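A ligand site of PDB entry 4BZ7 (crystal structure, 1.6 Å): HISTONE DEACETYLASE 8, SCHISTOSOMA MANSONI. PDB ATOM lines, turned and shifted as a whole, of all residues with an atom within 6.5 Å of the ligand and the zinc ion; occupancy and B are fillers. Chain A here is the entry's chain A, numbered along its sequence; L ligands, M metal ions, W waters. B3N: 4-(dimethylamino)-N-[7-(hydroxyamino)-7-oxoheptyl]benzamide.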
ATOM      1  N   PHE A  21     -17.298 -16.515   8.931  1.00  0.00           N
ATOM      2  CA  PHE A  21     -18.410 -15.879   8.195  1.00  0.00           C
ATOM      3  C   PHE A  21     -18.441 -14.370   8.197  1.00  0.00           C
ATOM      4  O   PHE A  21     -19.216 -13.784   7.450  1.00  0.00           O
ATOM      5  CB  PHE A  21     -19.748 -16.499   8.610  1.00  0.00           C
ATOM      6  CG  PHE A  21     -19.836 -17.936   8.188  1.00  0.00           C
ATOM      7  CD1 PHE A  21     -20.035 -18.290   6.860  1.00  0.00           C
ATOM      8  CD2 PHE A  21     -19.619 -18.961   9.109  1.00  0.00           C
ATOM      9  CE1 PHE A  21     -20.105 -19.629   6.478  1.00  0.00           C
ATOM     10  CE2 PHE A  21     -19.661 -20.297   8.715  1.00  0.00           C
ATOM     11  CZ  PHE A  21     -19.893 -20.629   7.400  1.00  0.00           C
ATOM     12  N   TYR A  99      -8.706 -26.563  15.672  1.00  0.00           N
ATOM     13  CA  TYR A  99      -8.448 -26.566  14.242  1.00  0.00           C
ATOM     14  C   TYR A  99      -9.447 -25.693  13.455  1.00  0.00           C
ATOM     15  O   TYR A  99      -9.452 -24.472  13.666  1.00  0.00           O
ATOM     16  CB  TYR A  99      -8.333 -28.024  13.720  1.00  0.00           C
ATOM     17  CG  TYR A  99      -7.290 -28.835  14.469  1.00  0.00           C
ATOM     18  CD1 TYR A  99      -5.952 -28.450  14.463  1.00  0.00           C
ATOM     19  CD2 TYR A  99      -7.639 -29.963  15.197  1.00  0.00           C
ATOM     20  CE1 TYR A  99      -4.975 -29.191  15.140  1.00  0.00           C
ATOM     21  CE2 TYR A  99      -6.678 -30.686  15.919  1.00  0.00           C
ATOM     22  CZ  TYR A  99      -5.350 -30.292  15.883  1.00  0.00           C
ATOM     23  OH  TYR A  99      -4.378 -31.010  16.561  1.00  0.00           O
ATOM     24  N   ASP A 100     -10.323 -26.292  12.623  1.00  0.00           N
ATOM     25  CA  ASP A 100     -11.323 -25.541  11.840  1.00  0.00           C
ATOM     26  C   ASP A 100     -12.583 -25.053  12.616  1.00  0.00           C
ATOM     27  O   ASP A 100     -13.389 -24.291  12.077  1.00  0.00           O
ATOM     28  CB  ASP A 100     -11.677 -26.237  10.499  1.00  0.00           C
ATOM     29  CG  ASP A 100     -10.610 -26.135   9.419  1.00  0.00           C
ATOM     30  OD1 ASP A 100      -9.562 -25.470   9.666  1.00  0.00           O
ATOM     31  OD2 ASP A 100     -10.796 -26.719   8.332  1.00  0.00           O
ATOM     32  N   GLY A 139     -28.858 -22.631  10.197  1.00  0.00           N
ATOM     33  CA  GLY A 139     -28.571 -23.731   9.254  1.00  0.00           C
ATOM     34  C   GLY A 139     -27.256 -24.455   9.492  1.00  0.00           C
ATOM     35  O   GLY A 139     -26.709 -25.060   8.568  1.00  0.00           O
ATOM     36  N   HIS A 141     -25.722 -27.372  10.139  1.00  0.00           N
ATOM     37  CA  HIS A 141     -26.066 -28.774  10.066  1.00  0.00           C
ATOM     38  C   HIS A 141     -25.085 -29.826  10.568  1.00  0.00           C
ATOM     39  O   HIS A 141     -25.499 -30.959  10.765  1.00  0.00           O
ATOM     40  CB  HIS A 141     -26.573 -29.121   8.645  1.00  0.00           C
ATOM     41  CG  HIS A 141     -25.587 -28.905   7.517  1.00  0.00           C
ATOM     42  ND1 HIS A 141     -25.860 -29.375   6.246  1.00  0.00           N
ATOM     43  CD2 HIS A 141     -24.415 -28.228   7.481  1.00  0.00           C
ATOM     44  CE1 HIS A 141     -24.844 -29.016   5.485  1.00  0.00           C
ATOM     45  NE2 HIS A 141     -23.945 -28.314   6.177  1.00  0.00           N
ATOM     46  N   HIS A 142     -23.823 -29.461  10.759  1.00  0.00           N
ATOM     47  CA  HIS A 142     -22.813 -30.450  11.146  1.00  0.00           C
ATOM     48  C   HIS A 142     -22.626 -30.679  12.643  1.00  0.00           C
ATOM     49  O   HIS A 142     -21.981 -31.667  13.006  1.00  0.00           O
ATOM     50  CB  HIS A 142     -21.451 -30.064  10.561  1.00  0.00           C
ATOM     51  CG  HIS A 142     -21.435 -29.987   9.063  1.00  0.00           C
ATOM     52  ND1 HIS A 142     -21.760 -31.092   8.275  1.00  0.00           N
ATOM     53  CD2 HIS A 142     -21.060 -28.973   8.241  1.00  0.00           C
ATOM     54  CE1 HIS A 142     -21.606 -30.698   7.015  1.00  0.00           C
ATOM     55  NE2 HIS A 142     -21.171 -29.426   6.946  1.00  0.00           N
ATOM     56  N   SER A 149     -18.228 -29.286  14.503  1.00  0.00           N
ATOM     57  CA  SER A 149     -17.806 -29.857  13.219  1.00  0.00           C
ATOM     58  C   SER A 149     -18.112 -28.893  12.079  1.00  0.00           C
ATOM     59  O   SER A 149     -19.173 -28.252  12.111  1.00  0.00           O
ATOM     60  CB  SER A 149     -18.573 -31.160  12.961  1.00  0.00           C
ATOM     61  OG  SER A 149     -18.226 -31.707  11.694  1.00  0.00           O
ATOM     62  N   GLY A 150     -17.192 -28.741  11.136  1.00  0.00           N
ATOM     63  CA  GLY A 150     -17.451 -27.934   9.934  1.00  0.00           C
ATOM     64  C   GLY A 150     -17.946 -26.529  10.167  1.00  0.00           C
ATOM     65  O   GLY A 150     -18.893 -26.079   9.506  1.00  0.00           O
ATOM     66  N   PHE A 151     -17.302 -25.836  11.106  1.00  0.00           N
ATOM     67  CA  PHE A 151     -17.606 -24.445  11.491  1.00  0.00           C
ATOM     68  C   PHE A 151     -18.961 -24.322  12.206  1.00  0.00           C
ATOM     69  O   PHE A 151     -19.438 -23.199  12.392  1.00  0.00           O
ATOM     70  CB  PHE A 151     -17.497 -23.469  10.279  1.00  0.00           C
ATOM     71  CG  PHE A 151     -16.509 -23.797   9.149  1.00  0.00           C
ATOM     72  CD1 PHE A 151     -15.162 -24.043   9.432  1.00  0.00           C
ATOM     73  CD2 PHE A 151     -16.918 -23.815   7.827  1.00  0.00           C
ATOM     74  CE1 PHE A 151     -14.261 -24.350   8.407  1.00  0.00           C
ATOM     75  CE2 PHE A 151     -16.003 -24.102   6.790  1.00  0.00           C
ATOM     76  CZ  PHE A 151     -14.685 -24.368   7.087  1.00  0.00           C
ATOM     77  N   CYS A 152     -19.553 -25.459  12.637  1.00  0.00           N
ATOM     78  CA  CYS A 152     -20.853 -25.528  13.339  1.00  0.00           C
ATOM     79  C   CYS A 152     -20.593 -25.869  14.785  1.00  0.00           C
ATOM     80  O   CYS A 152     -19.992 -26.926  15.046  1.00  0.00           O
ATOM     81  CB  CYS A 152     -21.771 -26.582  12.712  1.00  0.00           C
ATOM     82  SG  CYS A 152     -22.113 -26.285  10.952  1.00  0.00           S
ATOM     83  N   ASP A 186     -27.380 -27.865   0.891  1.00  0.00           N
ATOM     84  CA  ASP A 186     -25.995 -27.451   0.987  1.00  0.00           C
ATOM     85  C   ASP A 186     -25.094 -28.390   0.163  1.00  0.00           C
ATOM     86  O   ASP A 186     -25.444 -29.553  -0.078  1.00  0.00           O
ATOM     87  CB  ASP A 186     -25.567 -27.564   2.465  1.00  0.00           C
ATOM     88  CG  ASP A 186     -24.303 -26.834   2.847  1.00  0.00           C
ATOM     89  OD1 ASP A 186     -23.212 -27.393   2.619  1.00  0.00           O
ATOM     90  OD2 ASP A 186     -24.400 -25.720   3.380  1.00  0.00           O
ATOM     91  N   LEU A 187     -23.945 -27.885  -0.279  1.00  0.00           N
ATOM     92  CA  LEU A 187     -22.968 -28.692  -1.005  1.00  0.00           C
ATOM     93  C   LEU A 187     -22.526 -29.925  -0.184  1.00  0.00           C
ATOM     94  O   LEU A 187     -22.194 -30.966  -0.771  1.00  0.00           O
ATOM     95  CB  LEU A 187     -21.727 -27.825  -1.285  1.00  0.00           C
ATOM     96  CG  LEU A 187     -20.581 -28.483  -2.077  1.00  0.00           C
ATOM     97  CD1 LEU A 187     -21.020 -28.865  -3.509  1.00  0.00           C
ATOM     98  CD2 LEU A 187     -19.407 -27.530  -2.150  1.00  0.00           C
ATOM     99  N   HIS A 188     -22.512 -29.771   1.140  1.00  0.00           N
ATOM    100  CA  HIS A 188     -22.075 -30.819   2.070  1.00  0.00           C
ATOM    101  C   HIS A 188     -23.209 -31.642   2.627  1.00  0.00           C
ATOM    102  O   HIS A 188     -24.328 -31.143   2.837  1.00  0.00           O
ATOM    103  CB  HIS A 188     -21.247 -30.208   3.216  1.00  0.00           C
ATOM    104  CG  HIS A 188     -20.055 -29.438   2.718  1.00  0.00           C
ATOM    105  ND1 HIS A 188     -20.157 -28.096   2.410  1.00  0.00           N
ATOM    106  CD2 HIS A 188     -18.804 -29.874   2.432  1.00  0.00           C
ATOM    107  CE1 HIS A 188     -18.934 -27.728   2.017  1.00  0.00           C
ATOM    108  NE2 HIS A 188     -18.094 -28.779   2.007  1.00  0.00           N
ATOM    109  N   HIS A 189     -22.892 -32.914   2.903  1.00  0.00           N
ATOM    110  CA  HIS A 189     -23.860 -33.824   3.542  1.00  0.00           C
ATOM    111  C   HIS A 189     -24.289 -33.251   4.917  1.00  0.00           C
ATOM    112  O   HIS A 189     -23.446 -32.891   5.727  1.00  0.00           O
ATOM    113  CB  HIS A 189     -23.214 -35.182   3.754  1.00  0.00           C
ATOM    114  CG  HIS A 189     -24.117 -36.157   4.457  1.00  0.00           C
ATOM    115  ND1 HIS A 189     -23.664 -36.897   5.547  1.00  0.00           N
ATOM    116  CD2 HIS A 189     -25.427 -36.459   4.234  1.00  0.00           C
ATOM    117  CE1 HIS A 189     -24.702 -37.647   5.923  1.00  0.00           C
ATOM    118  NE2 HIS A 189     -25.776 -37.427   5.147  1.00  0.00           N
ATOM    119  N   PHE A 216     -15.223 -33.507   2.682  1.00  0.00           N
ATOM    120  CA  PHE A 216     -15.916 -33.395   3.943  1.00  0.00           C
ATOM    121  C   PHE A 216     -17.452 -33.563   3.792  1.00  0.00           C
ATOM    122  O   PHE A 216     -18.018 -32.999   2.853  1.00  0.00           O
ATOM    123  CB  PHE A 216     -15.642 -31.987   4.486  1.00  0.00           C
ATOM    124  CG  PHE A 216     -16.230 -31.755   5.861  1.00  0.00           C
ATOM    125  CD1 PHE A 216     -15.555 -32.162   7.013  1.00  0.00           C
ATOM    126  CD2 PHE A 216     -17.507 -31.207   6.015  1.00  0.00           C
ATOM    127  CE1 PHE A 216     -16.098 -31.959   8.280  1.00  0.00           C
ATOM    128  CE2 PHE A 216     -18.050 -30.987   7.279  1.00  0.00           C
ATOM    129  CZ  PHE A 216     -17.355 -31.388   8.399  1.00  0.00           C
ATOM    130  N   GLN A 281     -32.540 -26.477   4.569  1.00  0.00           N
ATOM    131  CA  GLN A 281     -31.244 -25.845   4.762  1.00  0.00           C
ATOM    132  C   GLN A 281     -30.833 -25.436   3.349  1.00  0.00           C
ATOM    133  O   GLN A 281     -30.807 -26.264   2.438  1.00  0.00           O
ATOM    134  CB  GLN A 281     -30.272 -26.839   5.432  1.00  0.00           C
ATOM    135  CG  GLN A 281     -29.021 -26.167   6.021  1.00  0.00           C
ATOM    136  CD  GLN A 281     -27.883 -26.076   5.023  1.00  0.00           C
ATOM    137  OE1 GLN A 281     -28.067 -26.169   3.808  1.00  0.00           O
ATOM    138  NE2 GLN A 281     -26.664 -25.943   5.546  1.00  0.00           N
ATOM    139  N   GLY A 283     -27.862 -23.827   2.177  1.00  0.00           N
ATOM    140  CA  GLY A 283     -26.447 -23.436   2.079  1.00  0.00           C
ATOM    141  C   GLY A 283     -26.106 -23.095   0.645  1.00  0.00           C
ATOM    142  O   GLY A 283     -26.501 -23.827  -0.260  1.00  0.00           O
ATOM    143  N   ASP A 285     -23.250 -22.856  -0.980  1.00  0.00           N
ATOM    144  CA  ASP A 285     -21.950 -23.326  -1.490  1.00  0.00           C
ATOM    145  C   ASP A 285     -22.010 -24.198  -2.747  1.00  0.00           C
ATOM    146  O   ASP A 285     -20.964 -24.614  -3.271  1.00  0.00           O
ATOM    147  CB  ASP A 285     -21.071 -23.930  -0.362  1.00  0.00           C
ATOM    148  CG  ASP A 285     -21.780 -24.837   0.614  1.00  0.00           C
ATOM    149  OD1 ASP A 285     -22.964 -25.144   0.370  1.00  0.00           O
ATOM    150  OD2 ASP A 285     -21.125 -25.256   1.624  1.00  0.00           O
ATOM    151  N   HIS A 292     -15.467 -23.163  -3.341  1.00  0.00           N
ATOM    152  CA  HIS A 292     -15.311 -24.636  -3.410  1.00  0.00           C
ATOM    153  C   HIS A 292     -15.185 -25.061  -4.861  1.00  0.00           C
ATOM    154  O   HIS A 292     -14.488 -26.044  -5.167  1.00  0.00           O
ATOM    155  CB  HIS A 292     -16.511 -25.356  -2.807  1.00  0.00           C
ATOM    156  CG  HIS A 292     -16.445 -25.469  -1.320  1.00  0.00           C
ATOM    157  ND1 HIS A 292     -17.024 -24.513  -0.493  1.00  0.00           N
ATOM    158  CD2 HIS A 292     -15.880 -26.429  -0.543  1.00  0.00           C
ATOM    159  CE1 HIS A 292     -16.812 -24.939   0.742  1.00  0.00           C
ATOM    160  NE2 HIS A 292     -16.109 -26.063   0.769  1.00  0.00           N
ATOM    161  N   GLY A 338     -26.751 -21.519   5.872  1.00  0.00           N
ATOM    162  CA  GLY A 338     -25.742 -22.574   5.986  1.00  0.00           C
ATOM    163  C   GLY A 338     -24.460 -22.140   5.342  1.00  0.00           C
ATOM    164  O   GLY A 338     -24.039 -20.991   5.515  1.00  0.00           O
ATOM    165  N   GLY A 339     -23.812 -23.030   4.590  1.00  0.00           N
ATOM    166  CA  GLY A 339     -22.559 -22.672   3.929  1.00  0.00           C
ATOM    167  C   GLY A 339     -22.746 -21.584   2.894  1.00  0.00           C
ATOM    168  O   GLY A 339     -23.857 -21.223   2.534  1.00  0.00           O
ATOM    169  N   GLY A 340     -21.623 -21.037   2.441  1.00  0.00           N
ATOM    170  CA  GLY A 340     -21.673 -20.011   1.400  1.00  0.00           C
ATOM    171  C   GLY A 340     -20.532 -19.088   1.686  1.00  0.00           C
ATOM    172  O   GLY A 340     -20.622 -18.235   2.579  1.00  0.00           O
ATOM    173  N   TYR A 341     -19.453 -19.262   0.948  1.00  0.00           N
ATOM    174  CA  TYR A 341     -18.189 -18.618   1.171  1.00  0.00           C
ATOM    175  C   TYR A 341     -17.850 -17.471   0.240  1.00  0.00           C
ATOM    176  O   TYR A 341     -16.855 -16.785   0.444  1.00  0.00           O
ATOM    177  CB  TYR A 341     -17.106 -19.719   1.281  1.00  0.00           C
ATOM    178  CG  TYR A 341     -17.550 -20.760   2.296  1.00  0.00           C
ATOM    179  CD1 TYR A 341     -17.393 -20.540   3.658  1.00  0.00           C
ATOM    180  CD2 TYR A 341     -18.289 -21.881   1.896  1.00  0.00           C
ATOM    181  CE1 TYR A 341     -17.871 -21.449   4.598  1.00  0.00           C
ATOM    182  CE2 TYR A 341     -18.781 -22.789   2.836  1.00  0.00           C
ATOM    183  CZ  TYR A 341     -18.595 -22.549   4.185  1.00  0.00           C
ATOM    184  OH  TYR A 341     -19.078 -23.435   5.126  1.00  0.00           O
HETATM  185  O23 B3N L   1     -11.351 -31.736   7.617  1.00  0.00           O
HETATM  186  C13 B3N L   1     -10.808 -30.701   7.826  1.00  0.00           C
HETATM  187  C14 B3N L   1      -9.588 -30.680   8.675  1.00  0.00           C
HETATM  188  C15 B3N L   1      -8.805 -29.442   8.761  1.00  0.00           C
HETATM  189  C16 B3N L   1      -7.642 -29.416   9.537  1.00  0.00           C
HETATM  190  C17 B3N L   1      -7.228 -30.563  10.292  1.00  0.00           C
HETATM  191  N20 B3N L   1      -6.012 -30.536  11.099  1.00  0.00           N
HETATM  192  C22 B3N L   1      -5.121 -29.409  11.065  1.00  0.00           C
HETATM  193  C21 B3N L   1      -5.695 -31.638  12.007  1.00  0.00           C
HETATM  194  C18 B3N L   1      -7.996 -31.780  10.193  1.00  0.00           C
HETATM  195  C19 B3N L   1      -9.200 -31.795   9.437  1.00  0.00           C
HETATM  196  N12 B3N L   1     -11.320 -29.456   7.229  1.00  0.00           N
HETATM  197  C10 B3N L   1     -12.497 -29.463   6.374  1.00  0.00           C
HETATM  198  C9  B3N L   1     -13.676 -28.672   6.933  1.00  0.00           C
HETATM  199  C8  B3N L   1     -14.697 -28.181   5.901  1.00  0.00           C
HETATM  200  C7  B3N L   1     -16.089 -27.920   6.419  1.00  0.00           C
HETATM  201  C6  B3N L   1     -17.197 -27.624   5.380  1.00  0.00           C
HETATM  202  C5  B3N L   1     -18.351 -26.777   5.933  1.00  0.00           C
HETATM  203  C1  B3N L   1     -19.615 -26.579   5.122  1.00  0.00           C
HETATM  204  O2  B3N L   1     -19.713 -25.711   4.226  1.00  0.00           O
HETATM  205  N3  B3N L   1     -20.737 -27.353   5.455  1.00  0.00           N
HETATM  206  O4  B3N L   1     -21.849 -27.203   4.871  1.00  0.00           O
HETATM  207 ZN    ZN M   1     -21.432 -26.638   2.940  1.00  0.00          ZN
HETATM  208  O   HOH W   1     -20.562 -24.548   7.732  1.00  0.00           O
HETATM  209  O   HOH W   2     -22.953 -25.333   6.761  1.00  0.00           O
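OD2 of Asp 100 is in hydrogen-bond range of N12 of the ligand.
A ring nitrogen (NE2) of His 142 sits at hydrogen-bond distance from a nitrogen (N3) of the ligand (2.6 Å).
A nitrogen (N3) of the ligand sits at hydrogen-bond distance from a ring nitrogen (NE2) of His 141, at 3.4 Å.
OH of Tyr 341 sits close to O2 of the ligand.
The side-chain sulfur (SG) of Cys 152 is in hydrogen-bond range of the backbone NH (N) of His 142 (3.6 Å).
The side-chain amide nitrogen of Gln 281 is in hydrogen-bond range of the side-chain carboxylate of Asp 186.
A ring nitrogen (NE2) of His 142 sits at hydrogen-bond distance from a ring nitrogen (NE2) of His 141 (3.1 Å).
The side-chain carboxylate of Asp 285 is in hydrogen-bond range of the backbone NH of Leu 187, 3.0 Å away.
OD2 of Asp 186 lies within hydrogen-bond range of N of Gly 339, at 3.0 Å.
The backbone carbonyl oxygen (O) of Gly 150 is in hydrogen-bond range of the side-chain sulfur (SG) of Cys 152 (3.5 Å).
Tyr 99 touches the ligand.
Gly 150 touches the ligand.
Phe 151 touches the ligand (CE2 to C5, 3.7 Å).
CD2 of Phe 216 touches C7 of the ligand, at 3.6 Å.
Hydrophobic or aromatic side chains within 4 Å of the ligand: Tyr 99, His 141, His 142, Phe 151, His 188, Phe 216 and Tyr 341.
Within 4 Å of the ligand: Tyr 99, Asp 100, His 141, His 142, Gly 150, Phe 151, Asp 186, His 188, Phe 216, Asp 285 and Tyr 341.
The nearest printed residue that does not touch the ligand is Gly 339 (4.2 Å).
Of the 23 residues printed, 3 come within 4 Å of the zinc ion.
The zinc ion is bound by the side-chain carboxylate of Asp 285, the side-chain carboxylate of Asp 186, a ring nitrogen (ND1) of His 188, an oxygen (O4) of the ligand and an oxygen (O2) of the ligand.
Water W2 lies within hydrogen-bond range of NE2 of His 141, N3 of the ligand and N of Gly 339.
Water W1 lies within hydrogen-bond range of O of Gly 150 and OH of Tyr 341.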
